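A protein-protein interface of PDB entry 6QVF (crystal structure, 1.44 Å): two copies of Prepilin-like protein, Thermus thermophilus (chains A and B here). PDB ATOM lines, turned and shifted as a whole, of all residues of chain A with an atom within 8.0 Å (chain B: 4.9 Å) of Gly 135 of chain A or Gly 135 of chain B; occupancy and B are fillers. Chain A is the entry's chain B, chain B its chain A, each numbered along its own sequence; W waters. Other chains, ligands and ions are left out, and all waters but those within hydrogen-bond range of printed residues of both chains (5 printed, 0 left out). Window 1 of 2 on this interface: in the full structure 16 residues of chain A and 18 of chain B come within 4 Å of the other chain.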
ATOM      1  N   ALA A  18       0.538  21.070  -5.565  1.00  0.00           N
ATOM      2  CA  ALA A  18       1.187  22.261  -6.088  1.00  0.00           C
ATOM      3  C   ALA A  18       0.405  23.510  -5.671  1.00  0.00           C
ATOM      4  O   ALA A  18       1.030  24.510  -5.293  1.00  0.00           O
ATOM      5  CB  ALA A  18       1.308  22.190  -7.582  1.00  0.00           C
ATOM      6  N   LEU A  22       1.885  26.706  -3.621  1.00  0.00           N
ATOM      7  CA  LEU A  22       1.881  27.982  -4.298  1.00  0.00           C
ATOM      8  C   LEU A  22       1.113  29.029  -3.492  1.00  0.00           C
ATOM      9  O   LEU A  22       1.588  30.173  -3.352  1.00  0.00           O
ATOM     10  CB  LEU A  22       1.258  27.835  -5.688  1.00  0.00           C
ATOM     11  CG  LEU A  22       1.249  29.108  -6.528  1.00  0.00           C
ATOM     12  CD1 LEU A  22       2.657  29.516  -6.873  1.00  0.00           C
ATOM     13  CD2 LEU A  22       0.417  28.932  -7.792  1.00  0.00           C
ATOM     14  N   SER A  26       3.000  32.243  -1.882  1.00  0.00           N
ATOM     15  CA  SER A  26       2.553  33.553  -2.405  1.00  0.00           C
ATOM     16  C   SER A  26       2.027  34.425  -1.267  1.00  0.00           C
ATOM     17  O   SER A  26       2.256  35.622  -1.251  1.00  0.00           O
ATOM     18  CB  SER A  26       1.461  33.396  -3.460  1.00  0.00           C
ATOM     19  OG  SER A  26       1.963  32.675  -4.568  1.00  0.00           O
ATOM     20  N   ASP A 105       9.946  27.854  -5.214  1.00  0.00           N
ATOM     21  CA  ASP A 105      10.955  28.905  -5.298  1.00  0.00           C
ATOM     22  C   ASP A 105      10.260  30.262  -5.370  1.00  0.00           C
ATOM     23  O   ASP A 105       9.337  30.457  -6.178  1.00  0.00           O
ATOM     24  CB  ASP A 105      11.791  28.709  -6.571  1.00  0.00           C
ATOM     25  CG  ASP A 105      12.869  29.747  -6.769  1.00  0.00           C
ATOM     26  OD1 ASP A 105      12.554  30.841  -7.215  1.00  0.00           O
ATOM     27  OD2 ASP A 105      14.050  29.416  -6.480  1.00  0.00           O
ATOM     28  N   THR A 119       8.256  36.369  -8.541  1.00  0.00           N
ATOM     29  CA  THR A 119       7.626  35.139  -9.007  1.00  0.00           C
ATOM     30  C   THR A 119       7.715  34.046  -7.938  1.00  0.00           C
ATOM     31  O   THR A 119       8.713  33.912  -7.168  1.00  0.00           O
ATOM     32  CB  THR A 119       8.196  34.673 -10.344  1.00  0.00           C
ATOM     33  OG1 THR A 119       9.570  34.391 -10.121  1.00  0.00           O
ATOM     34  CG2 THR A 119       8.054  35.706 -11.439  1.00  0.00           C
ATOM     35  N   VAL A 120       6.652  33.227  -7.921  1.00  0.00           N
ATOM     36  CA  VAL A 120       6.569  32.057  -7.096  1.00  0.00           C
ATOM     37  C   VAL A 120       6.255  30.888  -8.043  1.00  0.00           C
ATOM     38  O   VAL A 120       5.278  30.935  -8.802  1.00  0.00           O
ATOM     39  CB  VAL A 120       5.506  32.173  -5.985  1.00  0.00           C
ATOM     40  CG1 VAL A 120       5.538  30.963  -5.051  1.00  0.00           C
ATOM     41  CG2 VAL A 120       5.626  33.496  -5.233  1.00  0.00           C
ATOM     42  N   VAL A 121       7.138  29.898  -8.064  1.00  0.00           N
ATOM     43  CA  VAL A 121       7.027  28.766  -8.972  1.00  0.00           C
ATOM     44  C   VAL A 121       7.130  27.480  -8.188  1.00  0.00           C
ATOM     45  O   VAL A 121       8.054  27.332  -7.399  1.00  0.00           O
ATOM     46  CB  VAL A 121       8.064  28.865 -10.094  1.00  0.00           C
ATOM     47  CG1 VAL A 121       7.942  27.722 -11.076  1.00  0.00           C
ATOM     48  CG2 VAL A 121       7.908  30.188 -10.797  1.00  0.00           C
ATOM     49  N   VAL A 122       6.247  26.524  -8.506  1.00  0.00           N
ATOM     50  CA  VAL A 122       6.237  25.242  -7.849  1.00  0.00           C
ATOM     51  C   VAL A 122       6.145  24.122  -8.877  1.00  0.00           C
ATOM     52  O   VAL A 122       5.506  24.268  -9.908  1.00  0.00           O
ATOM     53  CB  VAL A 122       5.096  25.134  -6.824  1.00  0.00           C
ATOM     54  CG1 VAL A 122       5.176  26.273  -5.814  1.00  0.00           C
ATOM     55  CG2 VAL A 122       3.737  25.063  -7.484  1.00  0.00           C
ATOM     56  N   THR A 123       6.761  23.002  -8.524  1.00  0.00           N
ATOM     57  CA  THR A 123       6.624  21.790  -9.323  1.00  0.00           C
ATOM     58  C   THR A 123       6.367  20.603  -8.399  1.00  0.00           C
ATOM     59  O   THR A 123       7.246  20.254  -7.571  1.00  0.00           O
ATOM     60  CB  THR A 123       7.858  21.536 -10.184  1.00  0.00           C
ATOM     61  OG1 THR A 123       8.079  22.569 -11.140  1.00  0.00           O
ATOM     62  CG2 THR A 123       7.762  20.223 -10.948  1.00  0.00           C
ATOM     63  N   VAL A 132       3.233  18.519 -12.108  1.00  0.00           N
ATOM     64  CA  VAL A 132       2.459  19.744 -12.326  1.00  0.00           C
ATOM     65  C   VAL A 132       3.294  20.953 -11.896  1.00  0.00           C
ATOM     66  O   VAL A 132       3.835  20.976 -10.764  1.00  0.00           O
ATOM     67  CB  VAL A 132       1.124  19.744 -11.573  1.00  0.00           C
ATOM     68  CG1 VAL A 132       0.403  21.079 -11.722  1.00  0.00           C
ATOM     69  CG2 VAL A 132       0.218  18.602 -12.035  1.00  0.00           C
ATOM     70  N   THR A 133       3.469  21.883 -12.831  1.00  0.00           N
ATOM     71  CA  THR A 133       4.234  23.128 -12.569  1.00  0.00           C
ATOM     72  C   THR A 133       3.313  24.332 -12.683  1.00  0.00           C
ATOM     73  O   THR A 133       2.709  24.571 -13.757  1.00  0.00           O
ATOM     74  CB  THR A 133       5.387  23.317 -13.561  1.00  0.00           C
ATOM     75  OG1 THR A 133       6.341  22.271 -13.355  1.00  0.00           O
ATOM     76  CG2 THR A 133       6.090  24.654 -13.420  1.00  0.00           C
ATOM     77  N   LEU A 134       3.237  25.107 -11.592  1.00  0.00           N
ATOM     78  CA  LEU A 134       2.406  26.287 -11.490  1.00  0.00           C
ATOM     79  C   LEU A 134       3.255  27.482 -11.055  1.00  0.00           C
ATOM     80  O   LEU A 134       4.203  27.347 -10.318  1.00  0.00           O
ATOM     81  CB  LEU A 134       1.291  26.095 -10.469  1.00  0.00           C
ATOM     82  CG  LEU A 134       0.381  24.896 -10.693  1.00  0.00           C
ATOM     83  CD1 LEU A 134      -0.576  24.757  -9.535  1.00  0.00           C
ATOM     84  CD2 LEU A 134      -0.383  25.001 -11.994  1.00  0.00           C
ATOM     85  N   GLY A 135       2.839  28.650 -11.497  1.00  0.00           N
ATOM     86  CA  GLY A 135       3.466  29.902 -11.146  1.00  0.00           C
ATOM     87  C   GLY A 135       2.453  30.961 -10.771  1.00  0.00           C
ATOM     88  O   GLY A 135       1.309  30.950 -11.196  1.00  0.00           O
ATOM     89  N   ARG A 136       2.910  31.892  -9.945  1.00  0.00           N
ATOM     90  CA  ARG A 136       2.181  33.098  -9.695  1.00  0.00           C
ATOM     91  C   ARG A 136       3.153  34.272  -9.790  1.00  0.00           C
ATOM     92  O   ARG A 136       4.267  34.201  -9.285  1.00  0.00           O
ATOM     93  CB  ARG A 136       1.477  33.065  -8.328  1.00  0.00           C
ATOM     94  CG  ARG A 136       0.705  34.335  -8.025  1.00  0.00           C
ATOM     95  CD  ARG A 136      -0.271  34.246  -6.855  1.00  0.00           C
ATOM     96  NE  ARG A 136      -0.925  35.534  -6.639  1.00  0.00           N
ATOM     97  CZ  ARG A 136      -1.586  35.857  -5.554  1.00  0.00           C
ATOM     98  NH1 ARG A 136      -1.758  34.925  -4.616  1.00  0.00           N
ATOM     99  NH2 ARG A 136      -1.979  37.127  -5.393  1.00  0.00           N
ATOM    100  N   ARG A 137       2.688  35.328 -10.437  1.00  0.00           N
ATOM    101  CA  ARG A 137       3.437  36.585 -10.602  1.00  0.00           C
ATOM    102  C   ARG A 137       2.812  37.643  -9.697  1.00  0.00           C
ATOM    103  O   ARG A 137       1.649  37.975  -9.877  1.00  0.00           O
ATOM    104  CB  ARG A 137       3.369  37.058 -12.050  1.00  0.00           C
ATOM    105  CG  ARG A 137       4.186  38.295 -12.355  1.00  0.00           C
ATOM    106  CD  ARG A 137       4.162  38.643 -13.824  1.00  0.00           C
ATOM    107  NE  ARG A 137       5.047  39.768 -14.202  1.00  0.00           N
ATOM    108  CZ  ARG A 137       4.654  41.026 -14.302  1.00  0.00           C
ATOM    109  NH1 ARG A 137       3.397  41.346 -14.043  1.00  0.00           N
ATOM    110  NH2 ARG A 137       5.528  41.936 -14.728  1.00  0.00           N
ATOM    111  N   VAL A 138       3.611  38.161  -8.773  1.00  0.00           N
ATOM    112  CA  VAL A 138       3.166  39.131  -7.795  1.00  0.00           C
ATOM    113  C   VAL A 138       3.947  40.421  -8.032  1.00  0.00           C
ATOM    114  O   VAL A 138       5.174  40.377  -8.100  1.00  0.00           O
ATOM    115  CB  VAL A 138       3.390  38.608  -6.361  1.00  0.00           C
ATOM    116  CG1 VAL A 138       2.852  39.587  -5.356  1.00  0.00           C
ATOM    117  CG2 VAL A 138       2.745  37.236  -6.118  1.00  0.00           C
ATOM    118  N   LEU B  22      -7.596  28.989 -15.817  1.00  0.00           N
ATOM    119  CA  LEU B  22      -6.333  28.301 -16.001  1.00  0.00           C
ATOM    120  C   LEU B  22      -6.589  26.803 -16.114  1.00  0.00           C
ATOM    121  O   LEU B  22      -6.000  26.120 -16.949  1.00  0.00           O
ATOM    122  CB  LEU B  22      -5.405  28.600 -14.843  1.00  0.00           C
ATOM    123  CG  LEU B  22      -4.015  27.995 -14.941  1.00  0.00           C
ATOM    124  CD1 LEU B  22      -3.216  28.561 -16.098  1.00  0.00           C
ATOM    125  CD2 LEU B  22      -3.259  28.169 -13.604  1.00  0.00           C
ATOM    126  N   VAL B 120       0.425  28.365 -20.243  1.00  0.00           N
ATOM    127  CA  VAL B 120      -0.900  28.887 -20.129  1.00  0.00           C
ATOM    128  C   VAL B 120      -0.841  29.932 -19.024  1.00  0.00           C
ATOM    129  O   VAL B 120      -0.402  29.622 -17.908  1.00  0.00           O
ATOM    130  CB  VAL B 120      -1.941  27.816 -19.779  1.00  0.00           C
ATOM    131  CG1 VAL B 120      -3.354  28.352 -19.765  1.00  0.00           C
ATOM    132  CG2 VAL B 120      -1.782  26.635 -20.727  1.00  0.00           C
ATOM    133  N   VAL B 121      -1.218  31.152 -19.370  1.00  0.00           N
ATOM    134  CA  VAL B 121      -1.070  32.294 -18.416  1.00  0.00           C
ATOM    135  C   VAL B 121      -2.381  33.052 -18.368  1.00  0.00           C
ATOM    136  O   VAL B 121      -2.987  33.355 -19.412  1.00  0.00           O
ATOM    137  CB  VAL B 121       0.117  33.198 -18.790  1.00  0.00           C
ATOM    138  CG1 VAL B 121       0.279  34.338 -17.812  1.00  0.00           C
ATOM    139  CG2 VAL B 121       1.376  32.378 -18.917  1.00  0.00           C
ATOM    140  N   THR B 133      -2.367  36.929 -11.250  1.00  0.00           N
ATOM    141  CA  THR B 133      -1.763  36.349 -12.466  1.00  0.00           C
ATOM    142  C   THR B 133      -1.189  34.984 -12.115  1.00  0.00           C
ATOM    143  O   THR B 133      -0.303  34.852 -11.243  1.00  0.00           O
ATOM    144  CB  THR B 133      -0.633  37.228 -13.026  1.00  0.00           C
ATOM    145  OG1 THR B 133      -1.184  38.460 -13.484  1.00  0.00           O
ATOM    146  CG2 THR B 133       0.138  36.587 -14.157  1.00  0.00           C
ATOM    147  N   LEU B 134      -1.691  33.957 -12.814  1.00  0.00           N
ATOM    148  CA  LEU B 134      -1.303  32.594 -12.619  1.00  0.00           C
ATOM    149  C   LEU B 134      -0.849  31.989 -13.941  1.00  0.00           C
ATOM    150  O   LEU B 134      -1.320  32.323 -14.992  1.00  0.00           O
ATOM    151  CB  LEU B 134      -2.459  31.741 -12.081  1.00  0.00           C
ATOM    152  CG  LEU B 134      -3.134  32.216 -10.796  1.00  0.00           C
ATOM    153  CD1 LEU B 134      -4.308  31.326 -10.425  1.00  0.00           C
ATOM    154  CD2 LEU B 134      -2.153  32.250  -9.638  1.00  0.00           C
ATOM    155  N   GLY B 135       0.075  31.065 -13.828  1.00  0.00           N
ATOM    156  CA  GLY B 135       0.577  30.302 -14.988  1.00  0.00           C
ATOM    157  C   GLY B 135       0.675  28.815 -14.714  1.00  0.00           C
ATOM    158  O   GLY B 135       0.793  28.350 -13.585  1.00  0.00           O
ATOM    159  N   ARG B 136       0.635  28.063 -15.808  1.00  0.00           N
ATOM    160  CA  ARG B 136       0.929  26.651 -15.784  1.00  0.00           C
ATOM    161  C   ARG B 136       1.833  26.314 -16.958  1.00  0.00           C
ATOM    162  O   ARG B 136       1.613  26.816 -18.080  1.00  0.00           O
ATOM    163  CB  ARG B 136      -0.323  25.792 -15.839  1.00  0.00           C
ATOM    164  CG  ARG B 136      -0.010  24.302 -15.778  1.00  0.00           C
ATOM    165  CD  ARG B 136      -1.211  23.440 -15.493  1.00  0.00           C
ATOM    166  NE  ARG B 136      -0.796  22.034 -15.517  1.00  0.00           N
ATOM    167  CZ  ARG B 136      -1.611  20.991 -15.553  1.00  0.00           C
ATOM    168  NH1 ARG B 136      -2.932  21.178 -15.549  1.00  0.00           N
ATOM    169  NH2 ARG B 136      -1.070  19.791 -15.731  1.00  0.00           N
ATOM    170  N   ARG B 137       2.885  25.561 -16.677  1.00  0.00           N
ATOM    171  CA  ARG B 137       3.838  25.126 -17.714  1.00  0.00           C
ATOM    172  C   ARG B 137       3.584  23.661 -18.003  1.00  0.00           C
ATOM    173  O   ARG B 137       3.691  22.851 -17.117  1.00  0.00           O
ATOM    174  CB  ARG B 137       5.269  25.332 -17.232  1.00  0.00           C
ATOM    175  CG  ARG B 137       6.335  24.915 -18.234  1.00  0.00           C
ATOM    176  CD  ARG B 137       7.701  25.178 -17.686  1.00  0.00           C
ATOM    177  NE  ARG B 137       8.792  24.969 -18.627  1.00  0.00           N
ATOM    178  CZ  ARG B 137       9.508  23.862 -18.735  1.00  0.00           C
ATOM    179  NH1 ARG B 137       9.230  22.815 -17.969  1.00  0.00           N
ATOM    180  NH2 ARG B 137      10.516  23.845 -19.601  1.00  0.00           N
HETATM  181  O   HOH W   1       1.120  40.142 -12.832  1.00  0.00           O
HETATM  182  O   HOH W   2       2.081  21.578 -15.325  1.00  0.00           O
HETATM  183  O   HOH W   3       7.263  21.994 -16.005  1.00  0.00           O
HETATM  184  O   HOH W   4      -0.758  37.335  -8.891  1.00  0.00           O
HETATM  185  O   HOH W   5      -0.825  28.768 -11.149  1.00  0.00           O
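O of Gly 135 of chain A is in hydrogen-bond range of N of Gly 135 of chain B, at 2.9 Å. The backbone NH (N) of Arg 137 of chain A lies within hydrogen-bond range of the backbone carbonyl oxygen (O) of Thr 133 of chain B (3.1 Å). N of Arg 137 of chain B sits at hydrogen-bond distance from O of Thr 133 of chain A (3.1 Å).
The backbone carbonyl oxygen of Val 120 of chain B lies within hydrogen-bond range of the backbone NH of Arg 136 of chain B, at 2.8 Å. The side-chain hydroxyl of Thr 133 of chain A is in hydrogen-bond range of the side-chain hydroxyl of Thr 123 of chain A, at 2.8 Å. The backbone NH of Val 122 of chain A lies within hydrogen-bond range of the backbone carbonyl oxygen of Leu 134 of chain A (2.9 Å). The backbone NH (N) of Arg 136 of chain A sits at hydrogen-bond distance from the backbone carbonyl oxygen (O) of Val 120 of chain A (2.8 Å).
Among the printed residues, merely in contact across the chains: Thr 133 of chain A with Arg 136 of chain B (3.4 Å), Leu 134 of chain A with Gly 135 of chain B (3.4 Å), Leu 134 of chain A with Arg 136 of chain B (3.9 Å), Gly 135 of chain A with Leu 134 of chain B (3.4 Å), Arg 136 of chain A with Thr 133 of chain B (3.4 Å) and Arg 136 of chain A with Leu 134 of chain B (3.9 Å).
Ser 26 of chain A touches none of the printed residues of chain B. Of the printed residues of chain B, Thr 133 of chain A touches Arg 136 and Arg 137. Of the printed residues of chain B, Leu 134 of chain A touches Gly 135 (3.4 Å) and Arg 136 (3.9 Å). Of chain B, only Leu 134 and Gly 135 come within 4 Å of Gly 135 of chain A. Printed residues of chain A within 4 Å of Gly 135 of chain B: Leu 134 and Gly 135. Of the printed residues of chain A, Arg 137 of chain B touches Thr 133. The nearest residue of chain B that does not touch Gly 135 of chain A is Thr 133 of chain B (4.2 Å). The nearest printed residue of chain B that does not touch Leu 134 of chain A is Leu 22 of chain B (4.6 Å).
Of the 8 printed residues of chain B, 5 touch a printed residue of chain A. Hydrophobic or aromatic side chains of chain B that line the printed part of chain A: Leu 134. Among the printed residues, 9 pairs touch across the chains.
Thr 133 of chain A touches Arg 136 of chain B, and with the chains exchanged Arg 136 of chain A touches Thr 133 of chain B. Thr 133 of chain A touches Arg 137 of chain B, and with the chains exchanged Arg 137 of chain A touches Thr 133 of chain B. Leu 134 of chain A touches Gly 135 of chain B, and with the chains exchanged Gly 135 of chain A touches Leu 134 of chain B. Leu 134 of chain A touches Arg 136 of chain B, and with the chains exchanged Arg 136 of chain A touches Leu 134 of chain B.
Water W4 lies within hydrogen-bond range of O of Arg 137 of chain A, N of Thr 133 of chain B and NE of Arg 136 of chain A. Water W2 lies within hydrogen-bond range of O of Arg 137 of chain B (2.7 Å), N of Thr 133 of chain A (2.9 Å) and NE of Arg 136 of chain B (2.9 Å). Water W3 bridges OG1 of Thr 133 of chain A (2.8 Å) and NH1 of Arg 137 of chain B (2.9 Å). Water W1 lies within hydrogen-bond range of the guanidinium group (NH1) of Arg 137 of chain A (2.8 Å) and the side-chain hydroxyl (OG1) of Thr 133 of chain B (2.9 Å). Water W5 lies within hydrogen-bond range of the backbone carbonyl oxygen of Gly 135 of chain B (3.0 Å) and the backbone carbonyl oxygen of Gly 135 of chain A (3.1 Å).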
